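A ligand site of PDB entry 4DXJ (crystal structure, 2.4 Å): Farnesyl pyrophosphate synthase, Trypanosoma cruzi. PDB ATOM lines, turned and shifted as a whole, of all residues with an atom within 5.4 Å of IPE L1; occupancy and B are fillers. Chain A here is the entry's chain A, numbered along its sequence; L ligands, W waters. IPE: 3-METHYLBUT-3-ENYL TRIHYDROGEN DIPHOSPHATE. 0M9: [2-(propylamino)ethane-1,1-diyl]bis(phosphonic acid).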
ATOM      1  N   GLY A  46      15.640  27.255   4.089  1.00  0.00           N
ATOM      2  CA  GLY A  46      16.340  28.530   4.061  1.00  0.00           C
ATOM      3  C   GLY A  46      17.675  28.549   4.797  1.00  0.00           C
ATOM      4  O   GLY A  46      18.444  29.495   4.673  1.00  0.00           O
ATOM      5  N   GLY A  47      17.931  27.513   5.586  1.00  0.00           N
ATOM      6  CA  GLY A  47      19.252  27.301   6.161  1.00  0.00           C
ATOM      7  C   GLY A  47      20.191  26.784   5.100  1.00  0.00           C
ATOM      8  O   GLY A  47      19.826  26.718   3.930  1.00  0.00           O
ATOM      9  N   LYS A  48      21.399  26.414   5.492  1.00  0.00           N
ATOM     10  CA  LYS A  48      22.376  25.973   4.487  1.00  0.00           C
ATOM     11  C   LYS A  48      22.493  24.446   4.443  1.00  0.00           C
ATOM     12  O   LYS A  48      23.271  23.886   3.673  1.00  0.00           O
ATOM     13  CB  LYS A  48      23.716  26.674   4.704  1.00  0.00           C
ATOM     14  CG  LYS A  48      23.579  28.209   4.877  1.00  0.00           C
ATOM     15  CD  LYS A  48      22.696  28.862   3.759  1.00  0.00           C
ATOM     16  CE  LYS A  48      21.831  30.027   4.290  1.00  0.00           C
ATOM     17  NZ  LYS A  48      22.544  31.346   4.269  1.00  0.00           N
ATOM     18  N   TYR A  49      21.661  23.807   5.268  1.00  0.00           N
ATOM     19  CA  TYR A  49      21.539  22.353   5.372  1.00  0.00           C
ATOM     20  C   TYR A  49      22.853  21.604   5.581  1.00  0.00           C
ATOM     21  O   TYR A  49      23.029  20.513   5.025  1.00  0.00           O
ATOM     22  CB  TYR A  49      20.806  21.778   4.139  1.00  0.00           C
ATOM     23  CG  TYR A  49      19.571  22.543   3.702  1.00  0.00           C
ATOM     24  CD1 TYR A  49      19.597  23.328   2.547  1.00  0.00           C
ATOM     25  CD2 TYR A  49      18.387  22.482   4.428  1.00  0.00           C
ATOM     26  CE1 TYR A  49      18.471  24.026   2.125  1.00  0.00           C
ATOM     27  CE2 TYR A  49      17.256  23.195   4.022  1.00  0.00           C
ATOM     28  CZ  TYR A  49      17.315  23.954   2.874  1.00  0.00           C
ATOM     29  OH  TYR A  49      16.196  24.659   2.466  1.00  0.00           O
ATOM     30  N   PHE A  50      23.777  22.187   6.353  1.00  0.00           N
ATOM     31  CA  PHE A  50      25.058  21.530   6.654  1.00  0.00           C
ATOM     32  C   PHE A  50      24.839  20.172   7.324  1.00  0.00           C
ATOM     33  O   PHE A  50      25.409  19.167   6.898  1.00  0.00           O
ATOM     34  CB  PHE A  50      25.955  22.385   7.562  1.00  0.00           C
ATOM     35  CG  PHE A  50      26.670  23.506   6.858  1.00  0.00           C
ATOM     36  CD1 PHE A  50      26.811  23.504   5.461  1.00  0.00           C
ATOM     37  CD2 PHE A  50      27.236  24.562   7.589  1.00  0.00           C
ATOM     38  CE1 PHE A  50      27.487  24.550   4.799  1.00  0.00           C
ATOM     39  CE2 PHE A  50      27.911  25.604   6.936  1.00  0.00           C
ATOM     40  CZ  PHE A  50      28.030  25.596   5.544  1.00  0.00           C
ATOM     41  N   ARG A  51      24.004  20.177   8.348  1.00  0.00           N
ATOM     42  CA  ARG A  51      23.671  18.970   9.107  1.00  0.00           C
ATOM     43  C   ARG A  51      23.070  17.892   8.222  1.00  0.00           C
ATOM     44  O   ARG A  51      23.602  16.779   8.137  1.00  0.00           O
ATOM     45  CB  ARG A  51      22.727  19.302  10.272  1.00  0.00           C
ATOM     46  CG  ARG A  51      23.436  19.791  11.524  1.00  0.00           C
ATOM     47  CD  ARG A  51      22.511  20.584  12.438  1.00  0.00           C
ATOM     48  NE  ARG A  51      22.404  21.947  11.931  1.00  0.00           N
ATOM     49  CZ  ARG A  51      22.846  23.035  12.545  1.00  0.00           C
ATOM     50  NH1 ARG A  51      23.412  22.967  13.734  1.00  0.00           N
ATOM     51  NH2 ARG A  51      22.700  24.198  11.970  1.00  0.00           N
ATOM     52  N   GLU A  88      17.570  18.137  10.369  1.00  0.00           N
ATOM     53  CA  GLU A  88      17.087  19.473   9.993  1.00  0.00           C
ATOM     54  C   GLU A  88      15.843  19.887  10.773  1.00  0.00           C
ATOM     55  O   GLU A  88      15.733  21.038  11.221  1.00  0.00           O
ATOM     56  CB  GLU A  88      16.797  19.531   8.492  1.00  0.00           C
ATOM     57  CG  GLU A  88      18.050  19.542   7.630  1.00  0.00           C
ATOM     58  CD  GLU A  88      18.875  20.800   7.843  1.00  0.00           C
ATOM     59  OE1 GLU A  88      18.280  21.897   7.900  1.00  0.00           O
ATOM     60  OE2 GLU A  88      20.119  20.691   7.947  1.00  0.00           O
ATOM     61  N   GLN A  91      16.755  20.634  14.419  1.00  0.00           N
ATOM     62  CA  GLN A  91      17.245  21.987  14.545  1.00  0.00           C
ATOM     63  C   GLN A  91      16.111  22.983  14.390  1.00  0.00           C
ATOM     64  O   GLN A  91      16.053  23.949  15.147  1.00  0.00           O
ATOM     65  CB  GLN A  91      18.342  22.278  13.543  1.00  0.00           C
ATOM     66  CG  GLN A  91      19.310  23.329  14.092  1.00  0.00           C
ATOM     67  CD  GLN A  91      19.804  24.240  13.028  1.00  0.00           C
ATOM     68  OE1 GLN A  91      19.737  23.932  11.842  1.00  0.00           O
ATOM     69  NE2 GLN A  91      20.313  25.387  13.438  1.00  0.00           N
ATOM     70  N   LEU A  95      15.682  25.922  16.996  1.00  0.00           N
ATOM     71  CA  LEU A  95      15.688  27.325  16.608  1.00  0.00           C
ATOM     72  C   LEU A  95      14.392  28.024  16.965  1.00  0.00           C
ATOM     73  O   LEU A  95      14.405  29.168  17.420  1.00  0.00           O
ATOM     74  CB  LEU A  95      16.019  27.500  15.124  1.00  0.00           C
ATOM     75  CG  LEU A  95      17.355  26.910  14.652  1.00  0.00           C
ATOM     76  CD1 LEU A  95      17.620  27.239  13.179  1.00  0.00           C
ATOM     77  CD2 LEU A  95      18.566  27.347  15.538  1.00  0.00           C
ATOM     78  N   ARG A 107      15.402  35.436  11.887  1.00  0.00           N
ATOM     79  CA  ARG A 107      16.046  34.168  11.626  1.00  0.00           C
ATOM     80  C   ARG A 107      15.948  33.889  10.133  1.00  0.00           C
ATOM     81  O   ARG A 107      14.860  33.926   9.556  1.00  0.00           O
ATOM     82  CB  ARG A 107      15.377  33.051  12.447  1.00  0.00           C
ATOM     83  CG  ARG A 107      15.767  31.627  12.034  1.00  0.00           C
ATOM     84  CD  ARG A 107      17.129  31.239  12.585  1.00  0.00           C
ATOM     85  NE  ARG A 107      17.138  31.254  14.044  1.00  0.00           N
ATOM     86  CZ  ARG A 107      18.222  31.064  14.791  1.00  0.00           C
ATOM     87  NH1 ARG A 107      19.414  30.827  14.228  1.00  0.00           N
ATOM     88  NH2 ARG A 107      18.112  31.108  16.111  1.00  0.00           N
ATOM     89  N   ARG A 108      17.102  33.639   9.516  1.00  0.00           N
ATOM     90  CA  ARG A 108      17.247  33.293   8.093  1.00  0.00           C
ATOM     91  C   ARG A 108      16.608  34.314   7.126  1.00  0.00           C
ATOM     92  O   ARG A 108      16.061  33.952   6.088  1.00  0.00           O
ATOM     93  CB  ARG A 108      16.801  31.844   7.832  1.00  0.00           C
ATOM     94  CG  ARG A 108      17.277  30.861   8.904  1.00  0.00           C
ATOM     95  CD  ARG A 108      17.542  29.453   8.389  1.00  0.00           C
ATOM     96  NE  ARG A 108      16.335  28.634   8.260  1.00  0.00           N
ATOM     97  CZ  ARG A 108      16.158  27.438   8.823  1.00  0.00           C
ATOM     98  NH1 ARG A 108      17.085  26.878   9.583  1.00  0.00           N
ATOM     99  NH2 ARG A 108      15.014  26.797   8.617  1.00  0.00           N
ATOM    100  N   THR A 208      25.406  22.488  21.273  1.00  0.00           N
ATOM    101  CA  THR A 208      25.704  22.582  19.851  1.00  0.00           C
ATOM    102  C   THR A 208      26.346  21.355  19.196  1.00  0.00           C
ATOM    103  O   THR A 208      25.845  20.869  18.174  1.00  0.00           O
ATOM    104  CB  THR A 208      26.571  23.831  19.551  1.00  0.00           C
ATOM    105  OG1 THR A 208      25.809  25.009  19.846  1.00  0.00           O
ATOM    106  CG2 THR A 208      27.002  23.861  18.085  1.00  0.00           C
ATOM    107  N   TYR A 211      24.362  17.658  18.291  1.00  0.00           N
ATOM    108  CA  TYR A 211      23.385  17.614  17.208  1.00  0.00           C
ATOM    109  C   TYR A 211      23.892  18.244  15.895  1.00  0.00           C
ATOM    110  O   TYR A 211      23.364  17.926  14.832  1.00  0.00           O
ATOM    111  CB  TYR A 211      22.054  18.230  17.637  1.00  0.00           C
ATOM    112  CG  TYR A 211      21.918  19.712  17.371  1.00  0.00           C
ATOM    113  CD1 TYR A 211      21.402  20.171  16.170  1.00  0.00           C
ATOM    114  CD2 TYR A 211      22.276  20.638  18.333  1.00  0.00           C
ATOM    115  CE1 TYR A 211      21.268  21.530  15.925  1.00  0.00           C
ATOM    116  CE2 TYR A 211      22.141  22.006  18.091  1.00  0.00           C
ATOM    117  CZ  TYR A 211      21.639  22.435  16.892  1.00  0.00           C
ATOM    118  OH  TYR A 211      21.506  23.781  16.654  1.00  0.00           O
ATOM    119  N   THR A 212      24.892  19.129  15.982  1.00  0.00           N
ATOM    120  CA  THR A 212      25.417  19.774  14.763  1.00  0.00           C
ATOM    121  C   THR A 212      26.492  18.922  14.100  1.00  0.00           C
ATOM    122  O   THR A 212      26.572  18.888  12.864  1.00  0.00           O
ATOM    123  CB  THR A 212      25.990  21.181  15.041  1.00  0.00           C
ATOM    124  OG1 THR A 212      24.994  21.993  15.649  1.00  0.00           O
ATOM    125  CG2 THR A 212      26.402  21.858  13.750  1.00  0.00           C
ATOM    126  N   PHE A 246      32.658  25.934  15.440  1.00  0.00           N
ATOM    127  CA  PHE A 246      31.393  26.370  14.836  1.00  0.00           C
ATOM    128  C   PHE A 246      30.672  27.422  15.684  1.00  0.00           C
ATOM    129  O   PHE A 246      30.298  28.466  15.190  1.00  0.00           O
ATOM    130  CB  PHE A 246      30.489  25.156  14.573  1.00  0.00           C
ATOM    131  CG  PHE A 246      29.178  25.493  13.915  1.00  0.00           C
ATOM    132  CD1 PHE A 246      28.050  25.789  14.671  1.00  0.00           C
ATOM    133  CD2 PHE A 246      29.059  25.499  12.521  1.00  0.00           C
ATOM    134  CE1 PHE A 246      26.837  26.089  14.060  1.00  0.00           C
ATOM    135  CE2 PHE A 246      27.840  25.804  11.889  1.00  0.00           C
ATOM    136  CZ  PHE A 246      26.729  26.099  12.658  1.00  0.00           C
ATOM    137  N   GLN A 247      30.497  27.121  16.967  1.00  0.00           N
ATOM    138  CA  GLN A 247      29.829  28.011  17.916  1.00  0.00           C
ATOM    139  C   GLN A 247      30.613  29.285  18.214  1.00  0.00           C
ATOM    140  O   GLN A 247      30.029  30.344  18.432  1.00  0.00           O
ATOM    141  CB  GLN A 247      29.551  27.254  19.212  1.00  0.00           C
ATOM    142  CG  GLN A 247      28.590  27.965  20.156  1.00  0.00           C
ATOM    143  CD  GLN A 247      27.242  28.259  19.509  1.00  0.00           C
ATOM    144  OE1 GLN A 247      26.603  27.367  18.953  1.00  0.00           O
ATOM    145  NE2 GLN A 247      26.801  29.503  19.612  1.00  0.00           N
ATOM    146  N   ASP A 250      29.838  31.386  15.407  1.00  0.00           N
ATOM    147  CA  ASP A 250      28.483  31.887  15.640  1.00  0.00           C
ATOM    148  C   ASP A 250      28.446  33.073  16.629  1.00  0.00           C
ATOM    149  O   ASP A 250      27.737  34.062  16.381  1.00  0.00           O
ATOM    150  CB  ASP A 250      27.591  30.764  16.164  1.00  0.00           C
ATOM    151  CG  ASP A 250      26.148  31.208  16.318  1.00  0.00           C
ATOM    152  OD1 ASP A 250      25.436  31.333  15.287  1.00  0.00           O
ATOM    153  OD2 ASP A 250      25.727  31.455  17.466  1.00  0.00           O
ATOM    154  N   LYS A 264      20.250  36.902  10.782  1.00  0.00           N
ATOM    155  CA  LYS A 264      19.677  37.043  12.124  1.00  0.00           C
ATOM    156  C   LYS A 264      20.194  38.312  12.794  1.00  0.00           C
ATOM    157  O   LYS A 264      21.171  38.894  12.339  1.00  0.00           O
ATOM    158  CB  LYS A 264      19.933  35.787  12.964  1.00  0.00           C
ATOM    159  CG  LYS A 264      21.342  35.234  12.894  1.00  0.00           C
ATOM    160  CD  LYS A 264      21.410  33.870  13.577  1.00  0.00           C
ATOM    161  CE  LYS A 264      22.826  33.559  14.025  1.00  0.00           C
ATOM    162  NZ  LYS A 264      22.968  32.142  14.455  1.00  0.00           N
ATOM    163  N   ARG A 360      32.681  29.224   5.987  1.00  0.00           N
ATOM    164  CA  ARG A 360      31.350  29.839   6.083  1.00  0.00           C
ATOM    165  C   ARG A 360      31.417  31.284   6.569  1.00  0.00           C
ATOM    166  O   ARG A 360      32.299  31.666   7.337  1.00  0.00           O
ATOM    167  CB  ARG A 360      30.400  29.008   6.959  1.00  0.00           C
ATOM    168  CG  ARG A 360      30.471  29.310   8.466  1.00  0.00           C
ATOM    169  CD  ARG A 360      29.722  28.267   9.269  1.00  0.00           C
ATOM    170  NE  ARG A 360      29.769  28.555  10.703  1.00  0.00           N
ATOM    171  CZ  ARG A 360      28.756  29.065  11.404  1.00  0.00           C
ATOM    172  NH1 ARG A 360      27.596  29.312  10.826  1.00  0.00           N
ATOM    173  NH2 ARG A 360      28.892  29.297  12.704  1.00  0.00           N
ATOM    174  N   LYS A 362      28.125  32.570   6.867  1.00  0.00           N
ATOM    175  CA  LYS A 362      26.663  32.509   6.977  1.00  0.00           C
ATOM    176  C   LYS A 362      25.854  33.549   6.204  1.00  0.00           C
ATOM    177  O   LYS A 362      25.015  33.201   5.358  1.00  0.00           O
ATOM    178  CB  LYS A 362      26.222  32.401   8.445  1.00  0.00           C
ATOM    179  CG  LYS A 362      26.148  30.976   8.922  1.00  0.00           C
ATOM    180  CD  LYS A 362      24.915  30.239   8.387  1.00  0.00           C
ATOM    181  CE  LYS A 362      24.940  28.718   8.663  1.00  0.00           C
ATOM    182  NZ  LYS A 362      25.711  27.963   7.629  1.00  0.00           N
HETATM  183  C1  IPE L   1      22.725  28.131  14.159  1.00  0.00           C
HETATM  184  O1  IPE L   1      22.835  27.059  13.233  1.00  0.00           O
HETATM  185  C2  IPE L   1      22.524  27.552  15.552  1.00  0.00           C
HETATM  186  C3  IPE L   1      23.789  26.885  16.073  1.00  0.00           C
HETATM  187  C4  IPE L   1      23.768  25.597  16.360  1.00  0.00           C
HETATM  188  C5  IPE L   1      25.042  27.673  16.296  1.00  0.00           C
HETATM  189  PA  IPE L   1      23.079  27.329  11.661  1.00  0.00           P
HETATM  190  O1A IPE L   1      23.817  26.145  11.102  1.00  0.00           O
HETATM  191  O2A IPE L   1      23.633  28.739  11.550  1.00  0.00           O
HETATM  192  O3A IPE L   1      21.541  27.343  11.119  1.00  0.00           O
HETATM  193  PB  IPE L   1      21.012  26.970   9.628  1.00  0.00           P
HETATM  194  O1B IPE L   1      22.215  26.620   8.757  1.00  0.00           O
HETATM  195  O2B IPE L   1      20.076  25.803   9.859  1.00  0.00           O
HETATM  196  O3B IPE L   1      20.271  28.238   9.292  1.00  0.00           O
HETATM  197  O1  0M9 L   2      21.500  30.614  15.984  1.00  0.00           O
HETATM  198  P1  0M9 L   2      21.573  31.291  17.325  1.00  0.00           P
HETATM  199  O3  0M9 L   2      22.808  32.146  17.494  1.00  0.00           O
HETATM  200  O2  0M9 L   2      20.304  32.004  17.692  1.00  0.00           O
HETATM  201  C9  0M9 L   2      21.574  29.986  18.611  1.00  0.00           C
HETATM  202  P2  0M9 L   2      22.537  30.418  20.110  1.00  0.00           P
HETATM  203  O4  0M9 L   2      22.990  29.121  20.742  1.00  0.00           O
HETATM  204  O5  0M9 L   2      23.680  31.319  19.677  1.00  0.00           O
HETATM  205  O6  0M9 L   2      21.440  31.086  20.897  1.00  0.00           O
HETATM  206  C8  0M9 L   2      22.001  28.559  18.267  1.00  0.00           C
HETATM  207  N1  0M9 L   2      21.238  27.700  19.154  1.00  0.00           N
HETATM  208  C7  0M9 L   2      21.250  26.276  18.957  1.00  0.00           C
HETATM  209  C6  0M9 L   2      20.317  25.621  19.965  1.00  0.00           C
HETATM  210  C5  0M9 L   2      20.985  24.399  20.509  1.00  0.00           C
HETATM  211  O   HOH W   1      21.642  30.149   7.808  1.00  0.00           O
HETATM  212  O   HOH W   2      20.063  30.302  11.234  1.00  0.00           O
HETATM  213  O   HOH W   3      25.871  30.148  13.235  1.00  0.00           O
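OD1 of Asp 250 is in salt-bridge range of NZ of Lys 264, 2.7 Å away. The guanidinium group (NH2) of Arg 360 lies within hydrogen-bond range of the backbone carbonyl oxygen (O) of Phe 246. OG1 of Thr 212 lies within hydrogen-bond range of NH1 of Arg 51 (2.7 Å). O of Lys 362 lies within hydrogen-bond range of NZ of Lys 48, at 3.3 Å. The guanidinium group (NH2) of Arg 51 lies within hydrogen-bond range of the side-chain amide oxygen (OE1) of Gln 91 (3.0 Å). The side-chain carboxylate (OD2) of Asp 250 sits close to the side-chain amide nitrogen (NE2) of Gln 247 (3.1 Å). OE1 of Gln 247 sits at hydrogen-bond distance from OG1 of Thr 208 (2.6 Å). OG1 of Thr 212 lies within hydrogen-bond range of O of Thr 208 (2.9 Å).
O1B of IPE L1 is in hydrogen-bond range of N of Lys 48, at 3.4 Å. An oxygen (O2B) of IPE L1 sits close to the side-chain amide oxygen of Gln 91 (2.7 Å). NH2 of Arg 51 is in salt-bridge range of O1A of IPE L1. An oxygen (O1) of 0M9 L2 is in salt-bridge range of the side-chain amino group (NZ) of Lys 264 (2.6 Å). The guanidinium group of Arg 108 is in salt-bridge range of an oxygen (O2B) of IPE L1 (3.2 Å). NH1 of Arg 107 is in salt-bridge range of O1 of 0M9 L2 (2.7 Å). NZ of Lys 362 lies within salt-bridge range of O1B of IPE L1 (3.9 Å).
Residues that only touch IPE L1: Gly 47, Leu 95, Tyr 211, Thr 212, Phe 246, Gln 247 and Asp 250. Hydrophobic or aromatic side chains that line IPE L1: Leu 95, Tyr 211 and Phe 246. Of the 20 residues printed, 12 come within 4 Å of IPE L1. The nearest printed residue that does not touch IPE L1 is Lys 264 (4.03 Å).
Water W2 lies within hydrogen-bond range of an oxygen (O3B) of IPE L1 and the guanidinium group of Arg 107. Water W3 lies within hydrogen-bond range of OD1 of Asp 250 (2.4 Å), NH1 of Arg 360 (3.1 Å) and O2A of IPE L1 (3.1 Å).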
